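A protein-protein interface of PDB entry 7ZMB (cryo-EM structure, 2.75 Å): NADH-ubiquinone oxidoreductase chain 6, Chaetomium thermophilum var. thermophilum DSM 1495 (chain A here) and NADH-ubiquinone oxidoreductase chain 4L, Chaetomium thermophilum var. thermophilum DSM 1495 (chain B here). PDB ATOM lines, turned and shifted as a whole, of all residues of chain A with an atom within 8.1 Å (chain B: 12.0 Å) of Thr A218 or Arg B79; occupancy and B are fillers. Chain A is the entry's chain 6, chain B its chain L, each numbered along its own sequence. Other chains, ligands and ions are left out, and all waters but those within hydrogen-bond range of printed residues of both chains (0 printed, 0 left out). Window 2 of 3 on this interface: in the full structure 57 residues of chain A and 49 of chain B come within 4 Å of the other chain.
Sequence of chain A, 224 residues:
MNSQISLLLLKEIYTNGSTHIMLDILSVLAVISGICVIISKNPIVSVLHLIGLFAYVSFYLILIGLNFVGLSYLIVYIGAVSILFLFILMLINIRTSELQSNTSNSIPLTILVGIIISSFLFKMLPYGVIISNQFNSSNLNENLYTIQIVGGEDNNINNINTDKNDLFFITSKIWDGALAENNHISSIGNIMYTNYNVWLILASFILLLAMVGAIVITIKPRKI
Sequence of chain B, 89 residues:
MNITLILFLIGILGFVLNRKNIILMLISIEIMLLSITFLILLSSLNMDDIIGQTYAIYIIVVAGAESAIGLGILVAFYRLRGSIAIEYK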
ATOM      1  N   PHE A  87      11.188  29.913   5.938  1.00  0.00           N
ATOM      2  CA  PHE A  87      11.105  29.855   7.391  1.00  0.00           C
ATOM      3  C   PHE A  87       9.994  30.732   7.942  1.00  0.00           C
ATOM      4  O   PHE A  87       9.428  30.411   8.988  1.00  0.00           O
ATOM      5  CB  PHE A  87      12.447  30.233   8.004  1.00  0.00           C
ATOM      6  CG  PHE A  87      13.412  29.101   8.048  1.00  0.00           C
ATOM      7  CD1 PHE A  87      14.160  28.774   6.937  1.00  0.00           C
ATOM      8  CD2 PHE A  87      13.569  28.351   9.197  1.00  0.00           C
ATOM      9  CE1 PHE A  87      15.043  27.733   6.970  1.00  0.00           C
ATOM     10  CE2 PHE A  87      14.458  27.299   9.226  1.00  0.00           C
ATOM     11  CZ  PHE A  87      15.189  26.992   8.114  1.00  0.00           C
ATOM     12  N   MET A  90       6.839  28.629   7.956  1.00  0.00           N
ATOM     13  CA  MET A  90       6.815  27.605   8.991  1.00  0.00           C
ATOM     14  C   MET A  90       6.709  28.179  10.402  1.00  0.00           C
ATOM     15  O   MET A  90       6.074  27.564  11.260  1.00  0.00           O
ATOM     16  CB  MET A  90       8.069  26.739   8.860  1.00  0.00           C
ATOM     17  CG  MET A  90       8.232  25.671   9.903  1.00  0.00           C
ATOM     18  SD  MET A  90       9.511  24.506   9.432  1.00  0.00           S
ATOM     19  CE  MET A  90      10.947  25.568   9.398  1.00  0.00           C
ATOM     20  N   LEU A  91       7.304  29.343  10.667  1.00  0.00           N
ATOM     21  CA  LEU A  91       7.508  29.806  12.035  1.00  0.00           C
ATOM     22  C   LEU A  91       6.743  31.067  12.403  1.00  0.00           C
ATOM     23  O   LEU A  91       6.854  31.526  13.546  1.00  0.00           O
ATOM     24  CB  LEU A  91       8.999  30.057  12.297  1.00  0.00           C
ATOM     25  CG  LEU A  91       9.991  28.932  12.033  1.00  0.00           C
ATOM     26  CD1 LEU A  91      11.394  29.392  12.367  1.00  0.00           C
ATOM     27  CD2 LEU A  91       9.623  27.705  12.827  1.00  0.00           C
ATOM     28  N   MET A 211      27.458  23.824   9.201  1.00  0.00           N
ATOM     29  CA  MET A 211      26.890  22.572   8.628  1.00  0.00           C
ATOM     30  C   MET A 211      26.646  21.546   9.741  1.00  0.00           C
ATOM     31  O   MET A 211      25.629  20.853   9.678  1.00  0.00           O
ATOM     32  CB  MET A 211      27.814  21.975   7.561  1.00  0.00           C
ATOM     33  CG  MET A 211      27.948  22.814   6.313  1.00  0.00           C
ATOM     34  SD  MET A 211      29.130  22.119   5.132  1.00  0.00           S
ATOM     35  CE  MET A 211      28.200  20.717   4.518  1.00  0.00           C
ATOM     36  N   VAL A 212      27.544  21.459  10.720  1.00  0.00           N
ATOM     37  CA  VAL A 212      27.390  20.511  11.865  1.00  0.00           C
ATOM     38  C   VAL A 212      26.458  21.107  12.922  1.00  0.00           C
ATOM     39  O   VAL A 212      25.569  20.374  13.375  1.00  0.00           O
ATOM     40  CB  VAL A 212      28.756  20.120  12.468  1.00  0.00           C
ATOM     41  CG1 VAL A 212      28.617  19.335  13.763  1.00  0.00           C
ATOM     42  CG2 VAL A 212      29.607  19.362  11.466  1.00  0.00           C
ATOM     43  N   GLY A 213      26.635  22.378  13.288  1.00  0.00           N
ATOM     44  CA  GLY A 213      25.828  22.931  14.360  1.00  0.00           C
ATOM     45  C   GLY A 213      24.376  23.125  13.972  1.00  0.00           C
ATOM     46  O   GLY A 213      23.471  22.785  14.735  1.00  0.00           O
ATOM     47  N   ALA A 214      24.131  23.684  12.787  1.00  0.00           N
ATOM     48  CA  ALA A 214      22.756  23.950  12.381  1.00  0.00           C
ATOM     49  C   ALA A 214      21.945  22.670  12.248  1.00  0.00           C
ATOM     50  O   ALA A 214      20.713  22.723  12.283  1.00  0.00           O
ATOM     51  CB  ALA A 214      22.726  24.734  11.067  1.00  0.00           C
ATOM     52  N   ILE A 215      22.624  21.535  12.137  1.00  0.00           N
ATOM     53  CA  ILE A 215      21.930  20.229  11.961  1.00  0.00           C
ATOM     54  C   ILE A 215      21.797  19.554  13.326  1.00  0.00           C
ATOM     55  O   ILE A 215      20.764  18.921  13.561  1.00  0.00           O
ATOM     56  CB  ILE A 215      22.686  19.364  10.932  1.00  0.00           C
ATOM     57  CG1 ILE A 215      22.664  20.023   9.552  1.00  0.00           C
ATOM     58  CG2 ILE A 215      22.151  17.941  10.892  1.00  0.00           C
ATOM     59  CD1 ILE A 215      21.326  20.601   9.161  1.00  0.00           C
ATOM     60  N   VAL A 216      22.794  19.718  14.200  1.00  0.00           N
ATOM     61  CA  VAL A 216      22.761  19.083  15.549  1.00  0.00           C
ATOM     62  C   VAL A 216      21.544  19.617  16.312  1.00  0.00           C
ATOM     63  O   VAL A 216      20.905  18.817  17.010  1.00  0.00           O
ATOM     64  CB  VAL A 216      24.081  19.253  16.331  1.00  0.00           C
ATOM     65  CG1 VAL A 216      24.295  20.657  16.861  1.00  0.00           C
ATOM     66  CG2 VAL A 216      24.181  18.255  17.470  1.00  0.00           C
ATOM     67  N   ILE A 217      21.207  20.895  16.137  1.00  0.00           N
ATOM     68  CA  ILE A 217      20.123  21.511  16.956  1.00  0.00           C
ATOM     69  C   ILE A 217      18.737  21.334  16.332  1.00  0.00           C
ATOM     70  O   ILE A 217      17.761  21.621  17.042  1.00  0.00           O
ATOM     71  CB  ILE A 217      20.450  22.985  17.227  1.00  0.00           C
ATOM     72  CG1 ILE A 217      20.579  23.785  15.931  1.00  0.00           C
ATOM     73  CG2 ILE A 217      21.699  23.099  18.088  1.00  0.00           C
ATOM     74  CD1 ILE A 217      21.163  25.159  16.123  1.00  0.00           C
ATOM     75  N   THR A 218      18.643  20.898  15.072  1.00  0.00           N
ATOM     76  CA  THR A 218      17.307  20.827  14.419  1.00  0.00           C
ATOM     77  C   THR A 218      17.016  19.440  13.857  1.00  0.00           C
ATOM     78  O   THR A 218      16.008  19.317  13.160  1.00  0.00           O
ATOM     79  CB  THR A 218      17.188  21.824  13.264  1.00  0.00           C
ATOM     80  OG1 THR A 218      18.173  21.481  12.290  1.00  0.00           O
ATOM     81  CG2 THR A 218      17.353  23.263  13.692  1.00  0.00           C
ATOM     82  N   ILE A 219      17.791  18.432  14.216  1.00  0.00           N
ATOM     83  CA  ILE A 219      17.634  17.107  13.563  1.00  0.00           C
ATOM     84  C   ILE A 219      16.495  16.358  14.234  1.00  0.00           C
ATOM     85  O   ILE A 219      16.318  16.481  15.447  1.00  0.00           O
ATOM     86  CB  ILE A 219      18.953  16.302  13.567  1.00  0.00           C
ATOM     87  CG1 ILE A 219      18.945  15.187  12.519  1.00  0.00           C
ATOM     88  CG2 ILE A 219      19.308  15.782  14.949  1.00  0.00           C
ATOM     89  CD1 ILE A 219      18.662  15.679  11.124  1.00  0.00           C
ATOM     90  N   LYS A 220      15.736  15.620  13.439  1.00  0.00           N
ATOM     91  CA  LYS A 220      14.688  14.817  14.045  1.00  0.00           C
ATOM     92  C   LYS A 220      15.312  13.813  15.008  1.00  0.00           C
ATOM     93  O   LYS A 220      16.275  13.125  14.641  1.00  0.00           O
ATOM     94  CB  LYS A 220      13.875  14.087  12.976  1.00  0.00           C
ATOM     95  CG  LYS A 220      13.473  14.950  11.792  1.00  0.00           C
ATOM     96  CD  LYS A 220      12.424  15.983  12.168  1.00  0.00           C
ATOM     97  CE  LYS A 220      11.026  15.390  12.139  1.00  0.00           C
ATOM     98  NZ  LYS A 220       9.974  16.428  12.320  1.00  0.00           N
ATOM     99  N   PRO A 221      14.814  13.703  16.234  1.00  0.00           N
ATOM    100  CA  PRO A 221      15.428  12.779  17.196  1.00  0.00           C
ATOM    101  C   PRO A 221      14.931  11.352  17.029  1.00  0.00           C
ATOM    102  O   PRO A 221      13.787  11.037  17.370  1.00  0.00           O
ATOM    103  CB  PRO A 221      15.022  13.369  18.550  1.00  0.00           C
ATOM    104  CG  PRO A 221      13.750  14.133  18.278  1.00  0.00           C
ATOM    105  CD  PRO A 221      13.639  14.390  16.791  1.00  0.00           C
ATOM    106  N   ILE B  22      11.511  37.597  15.395  1.00  0.00           N
ATOM    107  CA  ILE B  22      12.954  37.396  15.411  1.00  0.00           C
ATOM    108  C   ILE B  22      13.534  37.149  14.021  1.00  0.00           C
ATOM    109  O   ILE B  22      14.736  37.356  13.819  1.00  0.00           O
ATOM    110  CB  ILE B  22      13.296  36.249  16.379  1.00  0.00           C
ATOM    111  CG1 ILE B  22      12.691  36.526  17.754  1.00  0.00           C
ATOM    112  CG2 ILE B  22      14.798  36.047  16.514  1.00  0.00           C
ATOM    113  CD1 ILE B  22      12.321  35.285  18.521  1.00  0.00           C
ATOM    114  N   ILE B  23      12.734  36.715  13.046  1.00  0.00           N
ATOM    115  CA  ILE B  23      13.272  36.644  11.690  1.00  0.00           C
ATOM    116  C   ILE B  23      13.589  38.045  11.183  1.00  0.00           C
ATOM    117  O   ILE B  23      14.572  38.244  10.466  1.00  0.00           O
ATOM    118  CB  ILE B  23      12.321  35.880  10.745  1.00  0.00           C
ATOM    119  CG1 ILE B  23      12.205  34.428  11.187  1.00  0.00           C
ATOM    120  CG2 ILE B  23      12.839  35.904   9.318  1.00  0.00           C
ATOM    121  CD1 ILE B  23      11.554  33.507  10.189  1.00  0.00           C
ATOM    122  N   LEU B  26      16.839  38.937  12.671  1.00  0.00           N
ATOM    123  CA  LEU B  26      17.906  38.283  11.931  1.00  0.00           C
ATOM    124  C   LEU B  26      18.072  38.868  10.531  1.00  0.00           C
ATOM    125  O   LEU B  26      19.171  38.825   9.972  1.00  0.00           O
ATOM    126  CB  LEU B  26      17.601  36.787  11.902  1.00  0.00           C
ATOM    127  CG  LEU B  26      18.232  35.750  10.991  1.00  0.00           C
ATOM    128  CD1 LEU B  26      19.672  35.480  11.361  1.00  0.00           C
ATOM    129  CD2 LEU B  26      17.406  34.493  11.107  1.00  0.00           C
ATOM    130  N   ALA B  65      26.680  31.913   6.914  1.00  0.00           N
ATOM    131  CA  ALA B  65      26.877  30.994   8.026  1.00  0.00           C
ATOM    132  C   ALA B  65      26.130  31.467   9.265  1.00  0.00           C
ATOM    133  O   ALA B  65      25.521  30.663   9.979  1.00  0.00           O
ATOM    134  CB  ALA B  65      28.366  30.838   8.322  1.00  0.00           C
ATOM    135  N   GLU B  66      26.165  32.773   9.533  1.00  0.00           N
ATOM    136  CA  GLU B  66      25.426  33.313  10.666  1.00  0.00           C
ATOM    137  C   GLU B  66      23.925  33.116  10.494  1.00  0.00           C
ATOM    138  O   GLU B  66      23.234  32.732  11.443  1.00  0.00           O
ATOM    139  CB  GLU B  66      25.753  34.795  10.851  1.00  0.00           C
ATOM    140  CG  GLU B  66      24.897  35.484  11.896  1.00  0.00           C
ATOM    141  CD  GLU B  66      25.210  36.953  12.045  1.00  0.00           C
ATOM    142  OE1 GLU B  66      25.616  37.579  11.047  1.00  0.00           O
ATOM    143  OE2 GLU B  66      25.053  37.482  13.163  1.00  0.00           O
ATOM    144  N   SER B  67      23.403  33.362   9.293  1.00  0.00           N
ATOM    145  CA  SER B  67      21.962  33.257   9.086  1.00  0.00           C
ATOM    146  C   SER B  67      21.475  31.814   9.079  1.00  0.00           C
ATOM    147  O   SER B  67      20.303  31.571   9.373  1.00  0.00           O
ATOM    148  CB  SER B  67      21.555  33.961   7.791  1.00  0.00           C
ATOM    149  OG  SER B  67      22.213  33.411   6.666  1.00  0.00           O
ATOM    150  N   ALA B  68      22.341  30.856   8.754  1.00  0.00           N
ATOM    151  CA  ALA B  68      21.970  29.454   8.905  1.00  0.00           C
ATOM    152  C   ALA B  68      21.982  29.035  10.370  1.00  0.00           C
ATOM    153  O   ALA B  68      21.072  28.338  10.829  1.00  0.00           O
ATOM    154  CB  ALA B  68      22.903  28.571   8.082  1.00  0.00           C
ATOM    155  N   ILE B  69      22.997  29.458  11.123  1.00  0.00           N
ATOM    156  CA  ILE B  69      23.035  29.156  12.549  1.00  0.00           C
ATOM    157  C   ILE B  69      21.884  29.848  13.261  1.00  0.00           C
ATOM    158  O   ILE B  69      21.298  29.302  14.202  1.00  0.00           O
ATOM    159  CB  ILE B  69      24.404  29.541  13.144  1.00  0.00           C
ATOM    160  CG1 ILE B  69      25.483  28.597  12.626  1.00  0.00           C
ATOM    161  CG2 ILE B  69      24.379  29.476  14.662  1.00  0.00           C
ATOM    162  CD1 ILE B  69      25.098  27.143  12.708  1.00  0.00           C
ATOM    163  N   GLY B  70      21.531  31.054  12.817  1.00  0.00           N
ATOM    164  CA  GLY B  70      20.388  31.732  13.398  1.00  0.00           C
ATOM    165  C   GLY B  70      19.080  31.012  13.133  1.00  0.00           C
ATOM    166  O   GLY B  70      18.307  30.753  14.054  1.00  0.00           O
ATOM    167  N   LEU B  71      18.820  30.669  11.870  1.00  0.00           N
ATOM    168  CA  LEU B  71      17.572  29.988  11.548  1.00  0.00           C
ATOM    169  C   LEU B  71      17.491  28.629  12.225  1.00  0.00           C
ATOM    170  O   LEU B  71      16.398  28.190  12.601  1.00  0.00           O
ATOM    171  CB  LEU B  71      17.408  29.850  10.033  1.00  0.00           C
ATOM    172  CG  LEU B  71      17.035  31.132   9.288  1.00  0.00           C
ATOM    173  CD1 LEU B  71      17.108  30.928   7.806  1.00  0.00           C
ATOM    174  CD2 LEU B  71      15.652  31.606   9.688  1.00  0.00           C
ATOM    175  N   GLY B  72      18.627  27.954  12.390  1.00  0.00           N
ATOM    176  CA  GLY B  72      18.633  26.705  13.134  1.00  0.00           C
ATOM    177  C   GLY B  72      18.298  26.891  14.601  1.00  0.00           C
ATOM    178  O   GLY B  72      17.552  26.098  15.179  1.00  0.00           O
ATOM    179  N   ILE B  73      18.849  27.929  15.227  1.00  0.00           N
ATOM    180  CA  ILE B  73      18.550  28.195  16.628  1.00  0.00           C
ATOM    181  C   ILE B  73      17.116  28.670  16.782  1.00  0.00           C
ATOM    182  O   ILE B  73      16.428  28.324  17.750  1.00  0.00           O
ATOM    183  CB  ILE B  73      19.559  29.202  17.207  1.00  0.00           C
ATOM    184  CG1 ILE B  73      20.892  28.506  17.479  1.00  0.00           C
ATOM    185  CG2 ILE B  73      19.030  29.817  18.490  1.00  0.00           C
ATOM    186  CD1 ILE B  73      22.040  29.433  17.736  1.00  0.00           C
ATOM    187  N   LEU B  74      16.643  29.470  15.826  1.00  0.00           N
ATOM    188  CA  LEU B  74      15.273  29.962  15.855  1.00  0.00           C
ATOM    189  C   LEU B  74      14.273  28.813  15.804  1.00  0.00           C
ATOM    190  O   LEU B  74      13.278  28.811  16.537  1.00  0.00           O
ATOM    191  CB  LEU B  74      15.067  30.919  14.689  1.00  0.00           C
ATOM    192  CG  LEU B  74      13.905  31.898  14.668  1.00  0.00           C
ATOM    193  CD1 LEU B  74      13.670  32.508  16.046  1.00  0.00           C
ATOM    194  CD2 LEU B  74      14.220  32.961  13.644  1.00  0.00           C
ATOM    195  N   VAL B  75      14.509  27.822  14.954  1.00  0.00           N
ATOM    196  CA  VAL B  75      13.618  26.625  14.884  1.00  0.00           C
ATOM    197  C   VAL B  75      13.592  25.922  16.249  1.00  0.00           C
ATOM    198  O   VAL B  75      12.486  25.606  16.720  1.00  0.00           O
ATOM    199  CB  VAL B  75      14.002  25.673  13.734  1.00  0.00           C
ATOM    200  CG1 VAL B  75      13.412  24.284  13.895  1.00  0.00           C
ATOM    201  CG2 VAL B  75      13.624  26.253  12.386  1.00  0.00           C
ATOM    202  N   ALA B  76      14.768  25.644  16.826  1.00  0.00           N
ATOM    203  CA  ALA B  76      14.873  25.001  18.157  1.00  0.00           C
ATOM    204  C   ALA B  76      14.016  25.753  19.173  1.00  0.00           C
ATOM    205  O   ALA B  76      13.222  25.107  19.872  1.00  0.00           O
ATOM    206  CB  ALA B  76      16.318  24.931  18.568  1.00  0.00           C
ATOM    207  N   PHE B  77      14.190  27.069  19.251  1.00  0.00           N
ATOM    208  CA  PHE B  77      13.417  27.920  20.186  1.00  0.00           C
ATOM    209  C   PHE B  77      11.917  27.828  19.891  1.00  0.00           C
ATOM    210  O   PHE B  77      11.172  27.649  20.852  1.00  0.00           O
ATOM    211  CB  PHE B  77      13.946  29.355  20.064  1.00  0.00           C
ATOM    212  CG  PHE B  77      13.140  30.463  20.690  1.00  0.00           C
ATOM    213  CD1 PHE B  77      13.350  30.841  22.006  1.00  0.00           C
ATOM    214  CD2 PHE B  77      12.218  31.175  19.942  1.00  0.00           C
ATOM    215  CE1 PHE B  77      12.625  31.878  22.569  1.00  0.00           C
ATOM    216  CE2 PHE B  77      11.490  32.209  20.507  1.00  0.00           C
ATOM    217  CZ  PHE B  77      11.701  32.563  21.819  1.00  0.00           C
ATOM    218  N   TYR B  78      11.502  27.905  18.620  1.00  0.00           N
ATOM    219  CA  TYR B  78      10.064  27.865  18.232  1.00  0.00           C
ATOM    220  C   TYR B  78       9.437  26.520  18.602  1.00  0.00           C
ATOM    221  O   TYR B  78       8.293  26.495  19.031  1.00  0.00           O
ATOM    222  CB  TYR B  78       9.890  28.144  16.737  1.00  0.00           C
ATOM    223  CG  TYR B  78       8.482  28.051  16.208  1.00  0.00           C
ATOM    224  CD1 TYR B  78       7.974  26.854  15.732  1.00  0.00           C
ATOM    225  CD2 TYR B  78       7.664  29.166  16.159  1.00  0.00           C
ATOM    226  CE1 TYR B  78       6.687  26.762  15.238  1.00  0.00           C
ATOM    227  CE2 TYR B  78       6.376  29.094  15.660  1.00  0.00           C
ATOM    228  CZ  TYR B  78       5.887  27.887  15.198  1.00  0.00           C
ATOM    229  OH  TYR B  78       4.617  27.807  14.711  1.00  0.00           O
ATOM    230  N   ARG B  79      10.170  25.430  18.433  1.00  0.00           N
ATOM    231  CA  ARG B  79       9.572  24.105  18.704  1.00  0.00           C
ATOM    232  C   ARG B  79       9.119  24.115  20.154  1.00  0.00           C
ATOM    233  O   ARG B  79       8.074  23.533  20.444  1.00  0.00           O
ATOM    234  CB  ARG B  79      10.573  22.978  18.458  1.00  0.00           C
ATOM    235  CG  ARG B  79      10.952  22.762  17.002  1.00  0.00           C
ATOM    236  CD  ARG B  79      11.309  21.305  16.798  1.00  0.00           C
ATOM    237  NE  ARG B  79      12.370  21.083  15.828  1.00  0.00           N
ATOM    238  CZ  ARG B  79      12.184  20.911  14.528  1.00  0.00           C
ATOM    239  NH1 ARG B  79      13.223  20.702  13.742  1.00  0.00           N
ATOM    240  NH2 ARG B  79      10.967  20.949  14.018  1.00  0.00           N
ATOM    241  N   LEU B  80       9.892  24.742  21.033  1.00  0.00           N
ATOM    242  CA  LEU B  80       9.546  24.712  22.466  1.00  0.00           C
ATOM    243  C   LEU B  80       8.614  25.870  22.864  1.00  0.00           C
ATOM    244  O   LEU B  80       7.581  25.584  23.483  1.00  0.00           O
ATOM    245  CB  LEU B  80      10.869  24.697  23.218  1.00  0.00           C
ATOM    246  CG  LEU B  80      11.724  23.458  22.964  1.00  0.00           C
ATOM    247  CD1 LEU B  80      13.166  23.687  23.378  1.00  0.00           C
ATOM    248  CD2 LEU B  80      11.153  22.242  23.670  1.00  0.00           C
ATOM    249  N   ARG B  81       8.912  27.104  22.458  1.00  0.00           N
ATOM    250  CA  ARG B  81       8.084  28.281  22.827  1.00  0.00           C
ATOM    251  C   ARG B  81       6.781  28.294  22.012  1.00  0.00           C
ATOM    252  O   ARG B  81       5.729  28.622  22.595  1.00  0.00           O
ATOM    253  CB  ARG B  81       8.874  29.579  22.643  1.00  0.00           C
ATOM    254  CG  ARG B  81       8.132  30.816  23.130  1.00  0.00           C
ATOM    255  CD  ARG B  81       9.029  31.777  23.881  1.00  0.00           C
ATOM    256  NE  ARG B  81      10.012  31.080  24.698  1.00  0.00           N
ATOM    257  CZ  ARG B  81       9.844  30.757  25.974  1.00  0.00           C
ATOM    258  NH1 ARG B  81       8.719  31.068  26.594  1.00  0.00           N
ATOM    259  NH2 ARG B  81      10.802  30.122  26.625  1.00  0.00           N
ATOM    260  N   GLY B  82       6.847  27.990  20.712  1.00  0.00           N
ATOM    261  CA  GLY B  82       5.653  27.991  19.843  1.00  0.00           C
ATOM    262  C   GLY B  82       5.352  29.316  19.165  1.00  0.00           C
ATOM    263  O   GLY B  82       4.462  29.341  18.302  1.00  0.00           O
ATOM    264  N   SER B  83       6.027  30.391  19.550  1.00  0.00           N
ATOM    265  CA  SER B  83       5.875  31.700  18.871  1.00  0.00           C
ATOM    266  C   SER B  83       7.268  32.302  18.750  1.00  0.00           C
ATOM    267  O   SER B  83       8.018  32.196  19.733  1.00  0.00           O
ATOM    268  CB  SER B  83       4.980  32.609  19.665  1.00  0.00           C
ATOM    269  OG  SER B  83       4.848  33.873  19.044  1.00  0.00           O
ATOM    270  N   ILE B  84       7.625  32.872  17.600  1.00  0.00           N
ATOM    271  CA  ILE B  84       8.933  33.593  17.528  1.00  0.00           C
ATOM    272  C   ILE B  84       8.585  35.070  17.475  1.00  0.00           C
ATOM    273  O   ILE B  84       9.417  35.861  17.024  1.00  0.00           O
ATOM    274  CB  ILE B  84       9.816  33.120  16.362  1.00  0.00           C
ATOM    275  CG1 ILE B  84       9.179  33.428  15.003  1.00  0.00           C
ATOM    276  CG2 ILE B  84      10.163  31.651  16.503  1.00  0.00           C
ATOM    277  CD1 ILE B  84      10.149  33.384  13.856  1.00  0.00           C
ATOM    278  N   ALA B  85       7.375  35.407  17.902  1.00  0.00           N
ATOM    279  CA  ALA B  85       6.930  36.786  17.983  1.00  0.00           C
ATOM    280  C   ALA B  85       7.498  37.398  19.251  1.00  0.00           C
ATOM    281  O   ALA B  85       7.490  36.763  20.312  1.00  0.00           O
ATOM    282  CB  ALA B  85       5.405  36.870  17.984  1.00  0.00           C
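The side-chain hydroxyl (OG1) of Thr A218 sits at hydrogen-bond distance from the backbone carbonyl oxygen (O) of Ala A214 (2.8 Å).
The backbone carbonyl oxygen (O) of Ile B84 is in hydrogen-bond range of the backbone NH (N) of Ile B22 (3.2 Å).
No residue of chain B comes within 4 Å of Ile A215.
Thr A218 touches two residues of chain B.
No residue of chain B comes within 4 Å of Ile A219.
No residue of chain B comes within 4 Å of Lys A220.
Of the printed residues of chain A, Gly B72 touches Ile A217 (3.7 Å) and Thr A218 (3.2 Å).
Of the printed residues of chain A, Ile B73 touches Ile A217.
Of the printed residues of chain A, Val B75 touches Phe A87 and Leu A91.
Of the printed residues of chain A, Arg B79 touches Thr A218.
The nearest residue of chain B that does not touch Thr A218 is Val B75 (4.1 Å).
Of the 14 printed residues of chain A, 6 touch a printed residue of chain B.
Hydrophobic or aromatic side chains of chain A that line the printed part of chain B: Phe A87, Leu A91, Ala A214 and Ile A217.
Of the 24 printed residues of chain B, 11 touch a printed residue of chain A.
Printed residues of chain B that touch a printed residue of chain A: Ile B23, Ala B68, Ile B69, Leu B71, Gly B72, Ile B73, Val B75, Ala B76, Tyr B78, Arg B79 and Ile B84.
Among the printed residues, no Asp or Glu carboxylate lies within 4 Å of a Lys or Arg side-chain nitrogen of the other chain.
The guanidinium group (NH1) of Arg B79 is in hydrogen-bond range of the backbone carbonyl oxygen (O) of Thr A218 (3.2 Å).
CG2 of Val B75 touches CE2 of Phe A87, at 3.4 Å.
Met A90 touches Tyr B78.
CD1 of Leu A91 touches CG2 of Val B75, 3.9 Å away.
Tyr B78 touches Leu A91.
Leu A91 touches Ile B84.
Ile B69 touches Ala A214 (CD1 to N, 3.6 Å).
Gly B72 touches Ile A217.
Ile A217 touches Ile B73 (CD1 to CG1, 3.6 Å).
Ile A217 touches Ala B76 (O to CB, 3.9 Å).
Thr A218 touches Gly B72 (CG2 to O, 3.2 Å).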
